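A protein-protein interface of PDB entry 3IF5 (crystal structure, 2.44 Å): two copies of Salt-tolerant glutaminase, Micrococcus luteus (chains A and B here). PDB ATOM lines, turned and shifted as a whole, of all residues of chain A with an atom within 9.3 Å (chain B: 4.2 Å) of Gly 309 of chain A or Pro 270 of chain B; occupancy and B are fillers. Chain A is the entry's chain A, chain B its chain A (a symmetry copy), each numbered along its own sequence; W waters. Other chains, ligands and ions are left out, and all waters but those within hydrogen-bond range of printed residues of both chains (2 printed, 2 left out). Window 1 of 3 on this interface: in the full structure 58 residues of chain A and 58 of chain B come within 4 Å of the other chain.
NH2 of Arg 336 of chain B sits close to NH2 of Arg 303 of chain A (2.5 Å). The side-chain carboxylate (OD1) of Asp 308 of chain A is in salt-bridge range of the guanidinium group (NH2) of Arg 336 of chain B, 2.7 Å away. The backbone carbonyl oxygen (O) of Gly 309 of chain A is in hydrogen-bond range of the guanidinium group (NH1) of Arg 336 of chain B, at 2.9 Å. O of Gly 271 of chain B is in hydrogen-bond range of OG of Ser 311 of chain A.
O of Arg 303 of chain A is in hydrogen-bond range of NH2 of Arg 272 of chain A (3.2 Å). The guanidinium group (NH2) of Arg 272 of chain A lies within salt-bridge range of the side-chain carboxylate (OD2) of Asp 308 of chain A. N of Met 307 of chain A is in hydrogen-bond range of ND1 of His 305 of chain A, at 3.0 Å. O of Ala 212 of chain B is in hydrogen-bond range of N of Gly 271 of chain B (2.6 Å).
Among the printed residues, pairs that only touch across the chains: Met 307 of chain A with Pro 270 of chain B, Asp 310 of chain A with Arg 336 of chain B, Met 307 of chain A with Leu 306 of chain B, Gly 309 of chain A with Pro 270 of chain B and Gly 309 of chain A with Gly 271 of chain B.
Printed residues of chain B within 4 Å of Arg 303 of chain A: Arg 336 (2.5 Å). Printed residues of chain B within 4 Å of Met 307 of chain A: Pro 270 and Leu 306. Printed residues of chain B within 4 Å of Asp 308 of chain A: Arg 336. Of chain B, only Pro 270, Gly 271 and Arg 336 come within 4 Å of Gly 309 of chain A. Of the printed residues of chain B, Ser 311 of chain A touches Gly 271 (2.8 Å). Leu 312 of chain A touches none of the printed residues of chain B. No residue of chain A comes within 4 Å of Ala 212 of chain B. Printed residues of chain A within 4 Å of Pro 270 of chain B: Met 307 (3.6 Å) and Gly 309 (3.8 Å). Of chain A, only Gly 309 (3.8 Å) and Ser 311 (2.8 Å) come within 4 Å of Gly 271 of chain B. Arg 272 of chain B touches none of the printed residues of chain A. Of the printed residues of chain A, Leu 306 of chain B touches Met 307 (3.7 Å). The nearest printed residue of chain B that does not touch Gly 309 of chain A is Ala 212 of chain B (5.0 Å). The nearest printed residue of chain A that does not touch Pro 270 of chain B is Leu 306 of chain A (4.02 Å). The nearest printed residue of chain B that does not touch Asp 310 of chain A is Gly 271 of chain B (4.6 Å).
Along chain B the printed residues that touch a printed residue of chain A span positions 270 to 336. Of the 13 printed residues of chain A, 6 touch a printed residue of chain B. Printed residues of chain A that touch a printed residue of chain B: Arg 303, Met 307, Asp 308, Gly 309, Asp 310 and Ser 311. Among the printed residues, 9 pairs touch across the chains. Among the printed residues, Asp or Glu carboxylates within 4 Å of a Lys or Arg side-chain nitrogen of the other chain: Asp 308 of chain A with Arg 336 of chain B.
Positions printed for both chains: 269, 270, 272 and 306. Of the 9 pairs that touch across the chains among the printed residues, none has its exchanged pair printed and touching as well.
Water W1 lies within hydrogen-bond range of N of Gly 309 of chain A and O of Ala 212 of chain B. Water W2 lies within hydrogen-bond range of OD1 of Asp 310 of chain A (2.6 Å) and N of Arg 336 of chain B (2.9 Å).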
ATOM      1  N   LEU A 269     -37.015   3.335 -10.964  1.00  0.00           N
ATOM      2  CA  LEU A 269     -35.634   3.458 -10.503  1.00  0.00           C
ATOM      3  C   LEU A 269     -35.545   2.875  -9.096  1.00  0.00           C
ATOM      4  O   LEU A 269     -35.957   3.504  -8.119  1.00  0.00           O
ATOM      5  CB  LEU A 269     -35.199   4.928 -10.498  1.00  0.00           C
ATOM      6  CG  LEU A 269     -33.697   5.216 -10.358  1.00  0.00           C
ATOM      7  CD1 LEU A 269     -32.913   4.420 -11.400  1.00  0.00           C
ATOM      8  CD2 LEU A 269     -33.445   6.710 -10.545  1.00  0.00           C
ATOM      9  N   PRO A 270     -34.990   1.660  -8.982  1.00  0.00           N
ATOM     10  CA  PRO A 270     -34.840   0.955  -7.706  1.00  0.00           C
ATOM     11  C   PRO A 270     -34.392   1.782  -6.504  1.00  0.00           C
ATOM     12  O   PRO A 270     -33.332   2.407  -6.524  1.00  0.00           O
ATOM     13  CB  PRO A 270     -33.870  -0.186  -8.045  1.00  0.00           C
ATOM     14  CG  PRO A 270     -33.158   0.300  -9.254  1.00  0.00           C
ATOM     15  CD  PRO A 270     -34.238   0.969 -10.043  1.00  0.00           C
ATOM     16  N   ARG A 272     -35.513   4.517  -5.454  1.00  0.00           N
ATOM     17  CA  ARG A 272     -35.756   5.939  -5.473  1.00  0.00           C
ATOM     18  C   ARG A 272     -37.120   6.435  -5.913  1.00  0.00           C
ATOM     19  O   ARG A 272     -37.740   7.178  -5.174  1.00  0.00           O
ATOM     20  CB  ARG A 272     -34.644   6.646  -6.251  1.00  0.00           C
ATOM     21  CG  ARG A 272     -33.314   6.591  -5.510  1.00  0.00           C
ATOM     22  CD  ARG A 272     -32.209   6.045  -6.388  1.00  0.00           C
ATOM     23  NE  ARG A 272     -31.490   7.120  -7.056  1.00  0.00           N
ATOM     24  CZ  ARG A 272     -30.600   6.937  -8.026  1.00  0.00           C
ATOM     25  NH1 ARG A 272     -30.317   5.712  -8.452  1.00  0.00           N
ATOM     26  NH2 ARG A 272     -29.982   7.982  -8.557  1.00  0.00           N
ATOM     27  N   ARG A 303     -30.468  13.993 -11.276  1.00  0.00           N
ATOM     28  CA  ARG A 303     -29.496  12.909 -11.191  1.00  0.00           C
ATOM     29  C   ARG A 303     -30.176  11.583 -10.868  1.00  0.00           C
ATOM     30  O   ARG A 303     -29.627  10.765 -10.135  1.00  0.00           O
ATOM     31  CB  ARG A 303     -28.429  13.193 -10.134  1.00  0.00           C
ATOM     32  CG  ARG A 303     -27.370  14.209 -10.540  1.00  0.00           C
ATOM     33  CD  ARG A 303     -26.172  14.109  -9.596  1.00  0.00           C
ATOM     34  NE  ARG A 303     -25.197  15.182  -9.776  1.00  0.00           N
ATOM     35  CZ  ARG A 303     -24.070  15.281  -9.085  1.00  0.00           C
ATOM     36  NH1 ARG A 303     -23.229  16.287  -9.294  1.00  0.00           N
ATOM     37  NH2 ARG A 303     -23.790  14.367  -8.190  1.00  0.00           N
ATOM     38  N   LEU A 304     -31.384  11.384 -11.390  1.00  0.00           N
ATOM     39  CA  LEU A 304     -32.089  10.126 -11.172  1.00  0.00           C
ATOM     40  C   LEU A 304     -31.543   9.137 -12.208  1.00  0.00           C
ATOM     41  O   LEU A 304     -32.164   8.880 -13.236  1.00  0.00           O
ATOM     42  CB  LEU A 304     -33.598  10.322 -11.340  1.00  0.00           C
ATOM     43  CG  LEU A 304     -34.282  11.094 -10.205  1.00  0.00           C
ATOM     44  CD1 LEU A 304     -35.746  11.315 -10.544  1.00  0.00           C
ATOM     45  CD2 LEU A 304     -34.144  10.323  -8.896  1.00  0.00           C
ATOM     46  N   HIS A 305     -30.367   8.596 -11.921  1.00  0.00           N
ATOM     47  CA  HIS A 305     -29.692   7.672 -12.822  1.00  0.00           C
ATOM     48  C   HIS A 305     -29.298   6.419 -12.056  1.00  0.00           C
ATOM     49  O   HIS A 305     -28.823   6.486 -10.926  1.00  0.00           O
ATOM     50  CB  HIS A 305     -28.446   8.360 -13.401  1.00  0.00           C
ATOM     51  CG  HIS A 305     -27.870   7.687 -14.607  1.00  0.00           C
ATOM     52  ND1 HIS A 305     -27.293   6.434 -14.565  1.00  0.00           N
ATOM     53  CD2 HIS A 305     -27.758   8.108 -15.889  1.00  0.00           C
ATOM     54  CE1 HIS A 305     -26.850   6.117 -15.769  1.00  0.00           C
ATOM     55  NE2 HIS A 305     -27.120   7.115 -16.593  1.00  0.00           N
ATOM     56  N   LEU A 306     -29.501   5.273 -12.686  1.00  0.00           N
ATOM     57  CA  LEU A 306     -29.172   3.994 -12.085  1.00  0.00           C
ATOM     58  C   LEU A 306     -27.720   3.958 -11.579  1.00  0.00           C
ATOM     59  O   LEU A 306     -27.442   3.425 -10.508  1.00  0.00           O
ATOM     60  CB  LEU A 306     -29.401   2.888 -13.123  1.00  0.00           C
ATOM     61  CG  LEU A 306     -29.620   1.453 -12.646  1.00  0.00           C
ATOM     62  CD1 LEU A 306     -30.797   1.388 -11.663  1.00  0.00           C
ATOM     63  CD2 LEU A 306     -29.889   0.573 -13.857  1.00  0.00           C
ATOM     64  N   MET A 307     -26.797   4.547 -12.333  1.00  0.00           N
ATOM     65  CA  MET A 307     -25.394   4.530 -11.943  1.00  0.00           C
ATOM     66  C   MET A 307     -25.021   5.568 -10.895  1.00  0.00           C
ATOM     67  O   MET A 307     -23.852   5.727 -10.547  1.00  0.00           O
ATOM     68  CB  MET A 307     -24.508   4.686 -13.180  1.00  0.00           C
ATOM     69  CG  MET A 307     -24.767   3.609 -14.240  1.00  0.00           C
ATOM     70  SD  MET A 307     -24.945   1.976 -13.493  1.00  0.00           S
ATOM     71  CE  MET A 307     -26.192   1.293 -14.491  1.00  0.00           C
ATOM     72  N   ASP A 308     -26.027   6.265 -10.387  1.00  0.00           N
ATOM     73  CA  ASP A 308     -25.817   7.285  -9.368  1.00  0.00           C
ATOM     74  C   ASP A 308     -26.162   6.675  -8.019  1.00  0.00           C
ATOM     75  O   ASP A 308     -27.328   6.640  -7.619  1.00  0.00           O
ATOM     76  CB  ASP A 308     -26.728   8.475  -9.634  1.00  0.00           C
ATOM     77  CG  ASP A 308     -26.381   9.663  -8.789  1.00  0.00           C
ATOM     78  OD1 ASP A 308     -25.321  10.276  -9.050  1.00  0.00           O
ATOM     79  OD2 ASP A 308     -27.161   9.973  -7.862  1.00  0.00           O
ATOM     80  N   GLY A 309     -25.146   6.193  -7.320  1.00  0.00           N
ATOM     81  CA  GLY A 309     -25.362   5.561  -6.034  1.00  0.00           C
ATOM     82  C   GLY A 309     -25.899   6.446  -4.929  1.00  0.00           C
ATOM     83  O   GLY A 309     -25.410   7.548  -4.691  1.00  0.00           O
ATOM     84  N   ASP A 310     -26.923   5.938  -4.252  1.00  0.00           N
ATOM     85  CA  ASP A 310     -27.562   6.625  -3.136  1.00  0.00           C
ATOM     86  C   ASP A 310     -27.876   5.531  -2.131  1.00  0.00           C
ATOM     87  O   ASP A 310     -28.802   4.748  -2.339  1.00  0.00           O
ATOM     88  CB  ASP A 310     -28.863   7.297  -3.587  1.00  0.00           C
ATOM     89  CG  ASP A 310     -29.553   8.040  -2.457  1.00  0.00           C
ATOM     90  OD1 ASP A 310     -28.934   8.956  -1.880  1.00  0.00           O
ATOM     91  OD2 ASP A 310     -30.713   7.712  -2.146  1.00  0.00           O
ATOM     92  N   SER A 311     -27.108   5.459  -1.051  1.00  0.00           N
ATOM     93  CA  SER A 311     -27.340   4.413  -0.063  1.00  0.00           C
ATOM     94  C   SER A 311     -27.161   4.856   1.380  1.00  0.00           C
ATOM     95  O   SER A 311     -26.421   5.793   1.675  1.00  0.00           O
ATOM     96  CB  SER A 311     -26.420   3.227  -0.343  1.00  0.00           C
ATOM     97  OG  SER A 311     -25.072   3.585  -0.114  1.00  0.00           O
ATOM     98  N   LEU A 312     -27.847   4.159   2.276  1.00  0.00           N
ATOM     99  CA  LEU A 312     -27.797   4.431   3.706  1.00  0.00           C
ATOM    100  C   LEU A 312     -26.358   4.404   4.211  1.00  0.00           C
ATOM    101  O   LEU A 312     -25.896   5.353   4.843  1.00  0.00           O
ATOM    102  CB  LEU A 312     -28.629   3.386   4.452  1.00  0.00           C
ATOM    103  CG  LEU A 312     -28.850   3.567   5.952  1.00  0.00           C
ATOM    104  CD1 LEU A 312     -29.574   4.884   6.214  1.00  0.00           C
ATOM    105  CD2 LEU A 312     -29.665   2.394   6.494  1.00  0.00           C
ATOM    106  N   ALA B 212     -17.631   3.292  -8.030  1.00  0.00           N
ATOM    107  CA  ALA B 212     -18.873   3.100  -7.290  1.00  0.00           C
ATOM    108  C   ALA B 212     -19.348   4.313  -6.482  1.00  0.00           C
ATOM    109  O   ALA B 212     -20.534   4.445  -6.194  1.00  0.00           O
ATOM    110  CB  ALA B 212     -18.735   1.892  -6.370  1.00  0.00           C
ATOM    111  N   ALA B 268     -17.923  -2.938  -9.822  1.00  0.00           N
ATOM    112  CA  ALA B 268     -18.221  -1.615  -9.272  1.00  0.00           C
ATOM    113  C   ALA B 268     -19.727  -1.420  -9.123  1.00  0.00           C
ATOM    114  O   ALA B 268     -20.407  -1.103 -10.093  1.00  0.00           O
ATOM    115  CB  ALA B 268     -17.657  -0.524 -10.181  1.00  0.00           C
ATOM    116  N   LEU B 269     -20.239  -1.612  -7.910  1.00  0.00           N
ATOM    117  CA  LEU B 269     -21.669  -1.453  -7.650  1.00  0.00           C
ATOM    118  C   LEU B 269     -21.894  -0.079  -7.028  1.00  0.00           C
ATOM    119  O   LEU B 269     -21.626   0.137  -5.845  1.00  0.00           O
ATOM    120  CB  LEU B 269     -22.168  -2.553  -6.704  1.00  0.00           C
ATOM    121  CG  LEU B 269     -23.687  -2.737  -6.581  1.00  0.00           C
ATOM    122  CD1 LEU B 269     -24.308  -2.890  -7.969  1.00  0.00           C
ATOM    123  CD2 LEU B 269     -23.983  -3.975  -5.737  1.00  0.00           C
ATOM    124  N   PRO B 270     -22.402   0.868  -7.830  1.00  0.00           N
ATOM    125  CA  PRO B 270     -22.667   2.242  -7.394  1.00  0.00           C
ATOM    126  C   PRO B 270     -23.288   2.424  -6.012  1.00  0.00           C
ATOM    127  O   PRO B 270     -24.366   1.903  -5.727  1.00  0.00           O
ATOM    128  CB  PRO B 270     -23.539   2.810  -8.524  1.00  0.00           C
ATOM    129  CG  PRO B 270     -24.127   1.602  -9.159  1.00  0.00           C
ATOM    130  CD  PRO B 270     -22.995   0.627  -9.157  1.00  0.00           C
ATOM    131  N   GLY B 271     -22.570   3.168  -5.167  1.00  0.00           N
ATOM    132  CA  GLY B 271     -23.022   3.463  -3.825  1.00  0.00           C
ATOM    133  C   GLY B 271     -22.810   2.353  -2.817  1.00  0.00           C
ATOM    134  O   GLY B 271     -22.990   2.553  -1.615  1.00  0.00           O
ATOM    135  N   ARG B 272     -22.421   1.170  -3.271  1.00  0.00           N
ATOM    136  CA  ARG B 272     -22.242   0.122  -2.296  1.00  0.00           C
ATOM    137  C   ARG B 272     -20.859  -0.479  -2.124  1.00  0.00           C
ATOM    138  O   ARG B 272     -20.364  -0.499  -1.012  1.00  0.00           O
ATOM    139  CB  ARG B 272     -23.287  -0.974  -2.514  1.00  0.00           C
ATOM    140  CG  ARG B 272     -24.690  -0.493  -2.166  1.00  0.00           C
ATOM    141  CD  ARG B 272     -25.660  -0.735  -3.301  1.00  0.00           C
ATOM    142  NE  ARG B 272     -26.345  -2.009  -3.146  1.00  0.00           N
ATOM    143  CZ  ARG B 272     -27.108  -2.569  -4.078  1.00  0.00           C
ATOM    144  NH1 ARG B 272     -27.283  -1.968  -5.249  1.00  0.00           N
ATOM    145  NH2 ARG B 272     -27.706  -3.726  -3.831  1.00  0.00           N
ATOM    146  N   LEU B 306     -27.584  -4.542  -8.724  1.00  0.00           N
ATOM    147  CA  LEU B 306     -27.922  -3.209  -9.187  1.00  0.00           C
ATOM    148  C   LEU B 306     -29.420  -2.906  -9.011  1.00  0.00           C
ATOM    149  O   LEU B 306     -29.796  -1.803  -8.623  1.00  0.00           O
ATOM    150  CB  LEU B 306     -27.525  -3.085 -10.664  1.00  0.00           C
ATOM    151  CG  LEU B 306     -27.298  -1.696 -11.261  1.00  0.00           C
ATOM    152  CD1 LEU B 306     -26.241  -0.932 -10.452  1.00  0.00           C
ATOM    153  CD2 LEU B 306     -26.851  -1.853 -12.706  1.00  0.00           C
ATOM    154  N   ARG B 336     -28.920  13.490  -1.427  1.00  0.00           N
ATOM    155  CA  ARG B 336     -29.026  13.643  -2.864  1.00  0.00           C
ATOM    156  C   ARG B 336     -30.519  13.828  -3.099  1.00  0.00           C
ATOM    157  O   ARG B 336     -31.245  14.191  -2.174  1.00  0.00           O
ATOM    158  CB  ARG B 336     -28.511  12.386  -3.556  1.00  0.00           C
ATOM    159  CG  ARG B 336     -27.187  11.893  -2.987  1.00  0.00           C
ATOM    160  CD  ARG B 336     -26.449  11.060  -3.985  1.00  0.00           C
ATOM    161  NE  ARG B 336     -26.046  11.866  -5.041  1.00  0.00           N
ATOM    162  CZ  ARG B 336     -25.348  11.350  -6.037  1.00  0.00           C
ATOM    163  NH1 ARG B 336     -25.013  10.017  -6.211  1.00  0.00           N
ATOM    164  NH2 ARG B 336     -25.031  12.364  -7.354  1.00  0.00           N
HETATM  165  O   HOH W   1     -22.799   6.590  -6.577  1.00  0.00           O
HETATM  166  O   HOH W   2     -30.044  10.978  -0.596  1.00  0.00           O
